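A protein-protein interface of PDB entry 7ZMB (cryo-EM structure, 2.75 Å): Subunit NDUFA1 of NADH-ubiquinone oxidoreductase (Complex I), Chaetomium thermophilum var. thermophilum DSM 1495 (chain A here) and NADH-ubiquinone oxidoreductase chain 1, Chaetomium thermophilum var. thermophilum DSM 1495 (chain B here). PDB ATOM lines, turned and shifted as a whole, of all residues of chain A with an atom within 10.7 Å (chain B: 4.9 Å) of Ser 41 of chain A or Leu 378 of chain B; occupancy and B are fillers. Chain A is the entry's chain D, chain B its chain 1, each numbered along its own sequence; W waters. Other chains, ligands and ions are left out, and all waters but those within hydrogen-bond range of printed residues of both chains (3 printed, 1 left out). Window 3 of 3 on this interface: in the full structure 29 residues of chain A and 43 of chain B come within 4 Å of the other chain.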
ATOM      1  N   ARG A  29      -8.302   4.620 -23.110  1.00  0.00           N
ATOM      2  CA  ARG A  29      -9.348   4.146 -24.041  1.00  0.00           C
ATOM      3  C   ARG A  29      -9.001   4.591 -25.457  1.00  0.00           C
ATOM      4  O   ARG A  29      -9.481   3.946 -26.384  1.00  0.00           O
ATOM      5  CB  ARG A  29     -10.775   4.453 -23.553  1.00  0.00           C
ATOM      6  CG  ARG A  29     -11.387   3.324 -22.742  1.00  0.00           C
ATOM      7  CD  ARG A  29     -12.834   2.954 -22.992  1.00  0.00           C
ATOM      8  NE  ARG A  29     -13.771   4.065 -22.958  1.00  0.00           N
ATOM      9  CZ  ARG A  29     -14.363   4.541 -21.872  1.00  0.00           C
ATOM     10  NH1 ARG A  29     -15.203   5.552 -21.982  1.00  0.00           N
ATOM     11  NH2 ARG A  29     -14.107   4.027 -20.683  1.00  0.00           N
ATOM     12  N   HIS A  38     -12.865   6.746 -28.313  1.00  0.00           N
ATOM     13  CA  HIS A  38     -13.802   5.635 -28.006  1.00  0.00           C
ATOM     14  C   HIS A  38     -15.227   5.959 -28.453  1.00  0.00           C
ATOM     15  O   HIS A  38     -15.433   7.007 -29.056  1.00  0.00           O
ATOM     16  CB  HIS A  38     -13.747   5.424 -26.499  1.00  0.00           C
ATOM     17  CG  HIS A  38     -14.249   6.615 -25.752  1.00  0.00           C
ATOM     18  ND1 HIS A  38     -13.512   7.775 -25.628  1.00  0.00           N
ATOM     19  CD2 HIS A  38     -15.422   6.847 -25.129  1.00  0.00           C
ATOM     20  CE1 HIS A  38     -14.203   8.667 -24.957  1.00  0.00           C
ATOM     21  NE2 HIS A  38     -15.372   8.116 -24.632  1.00  0.00           N
ATOM     22  N   ARG A  39     -16.155   5.053 -28.182  1.00  0.00           N
ATOM     23  CA  ARG A  39     -17.583   5.290 -28.481  1.00  0.00           C
ATOM     24  C   ARG A  39     -18.372   5.422 -27.185  1.00  0.00           C
ATOM     25  O   ARG A  39     -18.010   4.765 -26.222  1.00  0.00           O
ATOM     26  CB  ARG A  39     -18.115   4.096 -29.268  1.00  0.00           C
ATOM     27  CG  ARG A  39     -17.384   3.839 -30.576  1.00  0.00           C
ATOM     28  CD  ARG A  39     -17.626   4.973 -31.544  1.00  0.00           C
ATOM     29  NE  ARG A  39     -19.044   5.131 -31.813  1.00  0.00           N
ATOM     30  CZ  ARG A  39     -19.705   4.457 -32.743  1.00  0.00           C
ATOM     31  NH1 ARG A  39     -19.071   3.571 -33.488  1.00  0.00           N
ATOM     32  NH2 ARG A  39     -20.995   4.667 -32.921  1.00  0.00           N
ATOM     33  N   TRP A  40     -19.403   6.255 -27.163  1.00  0.00           N
ATOM     34  CA  TRP A  40     -20.297   6.405 -25.991  1.00  0.00           C
ATOM     35  C   TRP A  40     -21.753   6.432 -26.451  1.00  0.00           C
ATOM     36  O   TRP A  40     -21.970   6.622 -27.656  1.00  0.00           O
ATOM     37  CB  TRP A  40     -19.945   7.658 -25.185  1.00  0.00           C
ATOM     38  CG  TRP A  40     -20.054   8.959 -25.915  1.00  0.00           C
ATOM     39  CD1 TRP A  40     -21.136   9.787 -25.957  1.00  0.00           C
ATOM     40  CD2 TRP A  40     -19.024   9.608 -26.680  1.00  0.00           C
ATOM     41  NE1 TRP A  40     -20.858  10.895 -26.707  1.00  0.00           N
ATOM     42  CE2 TRP A  40     -19.571  10.814 -27.166  1.00  0.00           C
ATOM     43  CE3 TRP A  40     -17.705   9.285 -27.014  1.00  0.00           C
ATOM     44  CZ2 TRP A  40     -18.842  11.697 -27.962  1.00  0.00           C
ATOM     45  CZ3 TRP A  40     -16.985  10.157 -27.798  1.00  0.00           C
ATOM     46  CH2 TRP A  40     -17.546  11.347 -28.263  1.00  0.00           C
ATOM     47  N   SER A  41     -22.697   6.247 -25.522  1.00  0.00           N
ATOM     48  CA  SER A  41     -24.148   6.276 -25.835  1.00  0.00           C
ATOM     49  C   SER A  41     -24.441   5.270 -26.947  1.00  0.00           C
ATOM     50  O   SER A  41     -25.091   5.652 -27.938  1.00  0.00           O
ATOM     51  CB  SER A  41     -24.610   7.666 -26.135  1.00  0.00           C
ATOM     52  OG  SER A  41     -24.295   8.525 -25.054  1.00  0.00           O
ATOM     53  N   VAL A  42     -23.974   4.038 -26.787  1.00  0.00           N
ATOM     54  CA  VAL A  42     -24.080   3.015 -27.868  1.00  0.00           C
ATOM     55  C   VAL A  42     -25.391   2.240 -27.758  1.00  0.00           C
ATOM     56  O   VAL A  42     -25.731   1.813 -26.645  1.00  0.00           O
ATOM     57  CB  VAL A  42     -22.867   2.067 -27.781  1.00  0.00           C
ATOM     58  CG1 VAL A  42     -22.979   0.882 -28.720  1.00  0.00           C
ATOM     59  CG2 VAL A  42     -21.554   2.804 -27.996  1.00  0.00           C
ATOM     60  N   ASP A  43     -26.100   2.073 -28.870  1.00  0.00           N
ATOM     61  CA  ASP A  43     -27.352   1.273 -28.901  1.00  0.00           C
ATOM     62  C   ASP A  43     -27.105  -0.045 -29.642  1.00  0.00           C
ATOM     63  O   ASP A  43     -25.955  -0.296 -30.021  1.00  0.00           O
ATOM     64  CB  ASP A  43     -28.531   2.084 -29.445  1.00  0.00           C
ATOM     65  CG  ASP A  43     -28.330   2.685 -30.827  1.00  0.00           C
ATOM     66  OD1 ASP A  43     -27.326   2.355 -31.477  1.00  0.00           O
ATOM     67  OD2 ASP A  43     -29.194   3.478 -31.244  1.00  0.00           O
ATOM     68  N   GLN A  44     -28.151  -0.852 -29.812  1.00  0.00           N
ATOM     69  CA  GLN A  44     -28.042  -2.155 -30.504  1.00  0.00           C
ATOM     70  C   GLN A  44     -27.511  -1.957 -31.923  1.00  0.00           C
ATOM     71  O   GLN A  44     -26.782  -2.835 -32.387  1.00  0.00           O
ATOM     72  CB  GLN A  44     -29.394  -2.869 -30.465  1.00  0.00           C
ATOM     73  CG  GLN A  44     -29.344  -4.322 -30.917  1.00  0.00           C
ATOM     74  CD  GLN A  44     -28.256  -5.131 -30.250  1.00  0.00           C
ATOM     75  OE1 GLN A  44     -27.598  -5.952 -30.882  1.00  0.00           O
ATOM     76  NE2 GLN A  44     -28.055  -4.910 -28.960  1.00  0.00           N
ATOM     77  N   TRP A  45     -27.818  -0.825 -32.553  1.00  0.00           N
ATOM     78  CA  TRP A  45     -27.356  -0.545 -33.929  1.00  0.00           C
ATOM     79  C   TRP A  45     -25.832  -0.449 -33.907  1.00  0.00           C
ATOM     80  O   TRP A  45     -25.186  -1.150 -34.685  1.00  0.00           O
ATOM     81  CB  TRP A  45     -27.988   0.746 -34.447  1.00  0.00           C
ATOM     82  CG  TRP A  45     -27.607   1.103 -35.849  1.00  0.00           C
ATOM     83  CD1 TRP A  45     -26.476   1.744 -36.259  1.00  0.00           C
ATOM     84  CD2 TRP A  45     -28.378   0.854 -37.037  1.00  0.00           C
ATOM     85  NE1 TRP A  45     -26.482   1.897 -37.617  1.00  0.00           N
ATOM     86  CE2 TRP A  45     -27.636   1.365 -38.122  1.00  0.00           C
ATOM     87  CE3 TRP A  45     -29.615   0.252 -37.289  1.00  0.00           C
ATOM     88  CZ2 TRP A  45     -28.094   1.289 -39.436  1.00  0.00           C
ATOM     89  CZ3 TRP A  45     -30.065   0.176 -38.588  1.00  0.00           C
ATOM     90  CH2 TRP A  45     -29.311   0.685 -39.645  1.00  0.00           C
ATOM     91  N   ASP A  46     -25.296   0.401 -33.028  1.00  0.00           N
ATOM     92  CA  ASP A  46     -23.825   0.621 -32.984  1.00  0.00           C
ATOM     93  C   ASP A  46     -23.085  -0.646 -32.577  1.00  0.00           C
ATOM     94  O   ASP A  46     -22.025  -0.910 -33.149  1.00  0.00           O
ATOM     95  CB  ASP A  46     -23.495   1.799 -32.069  1.00  0.00           C
ATOM     96  CG  ASP A  46     -24.349   3.028 -32.317  1.00  0.00           C
ATOM     97  OD1 ASP A  46     -24.643   3.308 -33.490  1.00  0.00           O
ATOM     98  OD2 ASP A  46     -24.723   3.685 -31.331  1.00  0.00           O
ATOM     99  N   LYS A  47     -23.609  -1.352 -31.581  1.00  0.00           N
ATOM    100  CA  LYS A  47     -22.989  -2.615 -31.128  1.00  0.00           C
ATOM    101  C   LYS A  47     -22.916  -3.578 -32.312  1.00  0.00           C
ATOM    102  O   LYS A  47     -21.843  -4.176 -32.500  1.00  0.00           O
ATOM    103  CB  LYS A  47     -23.864  -3.210 -30.027  1.00  0.00           C
ATOM    104  CG  LYS A  47     -23.652  -2.663 -28.626  1.00  0.00           C
ATOM    105  CD  LYS A  47     -24.653  -3.222 -27.645  1.00  0.00           C
ATOM    106  CE  LYS A  47     -24.750  -2.403 -26.377  1.00  0.00           C
ATOM    107  NZ  LYS A  47     -25.223  -1.027 -26.653  1.00  0.00           N
ATOM    108  N   MET A  50     -20.306  -2.286 -34.916  1.00  0.00           N
ATOM    109  CA  MET A  50     -18.921  -2.542 -34.424  1.00  0.00           C
ATOM    110  C   MET A  50     -18.533  -3.996 -34.677  1.00  0.00           C
ATOM    111  O   MET A  50     -17.358  -4.259 -34.958  1.00  0.00           O
ATOM    112  CB  MET A  50     -18.726  -2.185 -32.945  1.00  0.00           C
ATOM    113  CG  MET A  50     -18.423  -0.716 -32.744  1.00  0.00           C
ATOM    114  SD  MET A  50     -18.260  -0.209 -31.023  1.00  0.00           S
ATOM    115  CE  MET A  50     -19.955  -0.363 -30.470  1.00  0.00           C
ATOM    116  N   ASP B 106     -20.675   3.247 -18.493  1.00  0.00           N
ATOM    117  CA  ASP B 106     -21.572   4.225 -19.171  1.00  0.00           C
ATOM    118  C   ASP B 106     -22.968   3.596 -19.214  1.00  0.00           C
ATOM    119  O   ASP B 106     -23.436   3.292 -20.319  1.00  0.00           O
ATOM    120  CB  ASP B 106     -21.031   4.704 -20.522  1.00  0.00           C
ATOM    121  CG  ASP B 106     -21.857   5.825 -21.135  1.00  0.00           C
ATOM    122  OD1 ASP B 106     -22.638   6.452 -20.388  1.00  0.00           O
ATOM    123  OD2 ASP B 106     -21.730   6.050 -22.353  1.00  0.00           O
ATOM    124  N   THR B 172     -23.797  10.870 -19.106  1.00  0.00           N
ATOM    125  CA  THR B 172     -23.145  11.572 -20.247  1.00  0.00           C
ATOM    126  C   THR B 172     -24.170  12.322 -21.105  1.00  0.00           C
ATOM    127  O   THR B 172     -23.856  13.439 -21.508  1.00  0.00           O
ATOM    128  CB  THR B 172     -22.230  10.664 -21.077  1.00  0.00           C
ATOM    129  OG1 THR B 172     -21.653  11.471 -22.102  1.00  0.00           O
ATOM    130  CG2 THR B 172     -22.952   9.500 -21.717  1.00  0.00           C
ATOM    131  N   VAL B 173     -25.331  11.727 -21.374  1.00  0.00           N
ATOM    132  CA  VAL B 173     -26.340  12.360 -22.267  1.00  0.00           C
ATOM    133  C   VAL B 173     -26.840  13.652 -21.625  1.00  0.00           C
ATOM    134  O   VAL B 173     -27.031  14.626 -22.348  1.00  0.00           O
ATOM    135  CB  VAL B 173     -27.487  11.394 -22.622  1.00  0.00           C
ATOM    136  CG1 VAL B 173     -28.518  12.057 -23.518  1.00  0.00           C
ATOM    137  CG2 VAL B 173     -26.969  10.120 -23.264  1.00  0.00           C
ATOM    138  N   GLU B 176     -24.199  16.163 -22.150  1.00  0.00           N
ATOM    139  CA  GLU B 176     -24.206  16.516 -23.594  1.00  0.00           C
ATOM    140  C   GLU B 176     -25.378  17.452 -23.900  1.00  0.00           C
ATOM    141  O   GLU B 176     -25.201  18.378 -24.695  1.00  0.00           O
ATOM    142  CB  GLU B 176     -24.182  15.228 -24.419  1.00  0.00           C
ATOM    143  CG  GLU B 176     -22.853  14.502 -24.342  1.00  0.00           C
ATOM    144  CD  GLU B 176     -21.683  15.314 -24.865  1.00  0.00           C
ATOM    145  OE1 GLU B 176     -20.577  15.178 -24.318  1.00  0.00           O
ATOM    146  OE2 GLU B 176     -21.881  16.073 -25.829  1.00  0.00           O
ATOM    147  N   SER B 177     -26.530  17.203 -23.286  1.00  0.00           N
ATOM    148  CA  SER B 177     -27.742  18.038 -23.494  1.00  0.00           C
ATOM    149  C   SER B 177     -27.477  19.478 -23.034  1.00  0.00           C
ATOM    150  O   SER B 177     -28.032  20.390 -23.647  1.00  0.00           O
ATOM    151  CB  SER B 177     -28.940  17.414 -22.816  1.00  0.00           C
ATOM    152  OG  SER B 177     -29.184  16.110 -23.310  1.00  0.00           O
ATOM    153  N   SER B 376     -31.220   7.165 -28.654  1.00  0.00           N
ATOM    154  CA  SER B 376     -29.791   7.428 -28.362  1.00  0.00           C
ATOM    155  C   SER B 376     -29.283   8.422 -29.407  1.00  0.00           C
ATOM    156  O   SER B 376     -29.437   8.147 -30.598  1.00  0.00           O
ATOM    157  CB  SER B 376     -29.008   6.155 -28.365  1.00  0.00           C
ATOM    158  OG  SER B 376     -29.647   5.174 -27.564  1.00  0.00           O
ATOM    159  N   LEU B 377     -28.766   9.563 -28.964  1.00  0.00           N
ATOM    160  CA  LEU B 377     -28.274  10.609 -29.897  1.00  0.00           C
ATOM    161  C   LEU B 377     -26.985  11.192 -29.330  1.00  0.00           C
ATOM    162  O   LEU B 377     -25.932  11.043 -29.973  1.00  0.00           O
ATOM    163  CB  LEU B 377     -29.354  11.683 -30.051  1.00  0.00           C
ATOM    164  CG  LEU B 377     -29.000  12.869 -30.944  1.00  0.00           C
ATOM    165  CD1 LEU B 377     -29.008  12.466 -32.410  1.00  0.00           C
ATOM    166  CD2 LEU B 377     -29.961  14.021 -30.701  1.00  0.00           C
ATOM    167  N   LEU B 378     -27.081  11.845 -28.175  1.00  0.00           N
ATOM    168  CA  LEU B 378     -25.896  12.495 -27.564  1.00  0.00           C
ATOM    169  C   LEU B 378     -25.281  11.532 -26.536  1.00  0.00           C
ATOM    170  O   LEU B 378     -24.118  11.164 -26.726  1.00  0.00           O
ATOM    171  CB  LEU B 378     -26.375  13.787 -26.891  1.00  0.00           C
ATOM    172  CG  LEU B 378     -27.178  14.747 -27.766  1.00  0.00           C
ATOM    173  CD1 LEU B 378     -27.819  15.835 -26.920  1.00  0.00           C
ATOM    174  CD2 LEU B 378     -26.299  15.368 -28.835  1.00  0.00           C
HETATM  175  O   HOH W   1     -21.940   3.772 -24.081  1.00  0.00           O
HETATM  176  O   HOH W   2     -24.971   8.400 -29.967  1.00  0.00           O
HETATM  177  O   HOH W   3     -32.026   4.598 -29.881  1.00  0.00           O
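Trp 40 of chain A touches Asp 106 of chain B.
Thr 172 of chain B touches Ser 41 of chain A.
Ser 41 of chain A touches Val 173 of chain B (OG to CG2, 3.6 Å).
Ser 41 of chain A touches Ser 376 of chain B.
Asp 43 of chain A touches Ser 376 of chain B (CB to OG, 3.8 Å).
OD2 of Asp 106 of chain B lies within hydrogen-bond range of N of Ser 41 of chain A (3.3 Å).
The side-chain hydroxyl (OG) of Ser 41 of chain A lies within hydrogen-bond range of the backbone carbonyl oxygen (O) of Leu 378 of chain B, 3.1 Å away.
O of Leu 378 of chain B lies within hydrogen-bond range of NE1 of Trp 40 of chain A, at 3.3 Å.
Water W2 bridges the backbone carbonyl oxygen (O) of Leu 377 of chain B and the backbone carbonyl oxygen (O) of Ser 41 of chain A.
Water W1 lies within hydrogen-bond range of the side-chain carboxylate (OD2) of Asp 106 of chain B (2.9 Å), the backbone NH (N) of Ser 41 of chain A (3.0 Å) and the backbone NH (N) of Val 42 of chain A (3.4 Å).
Water W3 bridges N of Ser 376 of chain B and OD2 of Asp 43 of chain A.
N of Trp 45 of chain A lies close to OD1 of Asp 43 of chain A (3.4 Å).
The side-chain carboxylate (OD1) of Asp 43 of chain A lies close to the backbone NH (N) of Asp 46 of chain A (3.2 Å).
The backbone carbonyl oxygen (O) of Val 173 of chain B is in hydrogen-bond range of the side-chain hydroxyl (OG) of Ser 177 of chain B (2.8 Å).
Printed residues of chain A that touch a printed residue of chain B: Trp 40, Ser 41 and Asp 43.
Hydrophobic or aromatic side chains of chain B within 4 Å of the printed part of chain A: Val 173.
Among the printed residues, 8 pairs touch across the chains.
Among the printed residues, no Asp or Glu carboxylate lies within 4 Å of a Lys or Arg side-chain nitrogen of the other chain.
Of chain B, only Asp 106, Thr 172, Val 173, Ser 376 and Leu 378 come within 4 Å of Ser 41 of chain A.
Of chain A, only Trp 40 (3.3 Å) and Ser 41 (3.1 Å) come within 4 Å of Leu 378 of chain B.
Of chain A, only Ser 41 comes within 4 Å of Thr 172 of chain B.
No residue of chain A comes within 4 Å of Glu 176 of chain B.
Ser 376 of chain B touches just these residues of chain A: Ser 41 and Asp 43.
No residue of chain A comes within 4 Å of Leu 377 of chain B.
Printed residues of chain B within 4 Å of Trp 40 of chain A: Asp 106 (3.7 Å) and Leu 378 (3.3 Å).
Of the printed residues of chain A, Asp 106 of chain B touches Trp 40 and Ser 41.
Of the printed residues of chain B, Asp 43 of chain A touches Ser 376.
Gln 44 of chain A touches none of the printed residues of chain B.
His 38 of chain A touches none of the printed residues of chain B.
The nearest printed residue of chain B that does not touch Ser 41 of chain A is Leu 377 of chain B (5.3 Å).
The nearest printed residue of chain B that does not touch Trp 40 of chain A is Thr 172 of chain B (4.2 Å).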
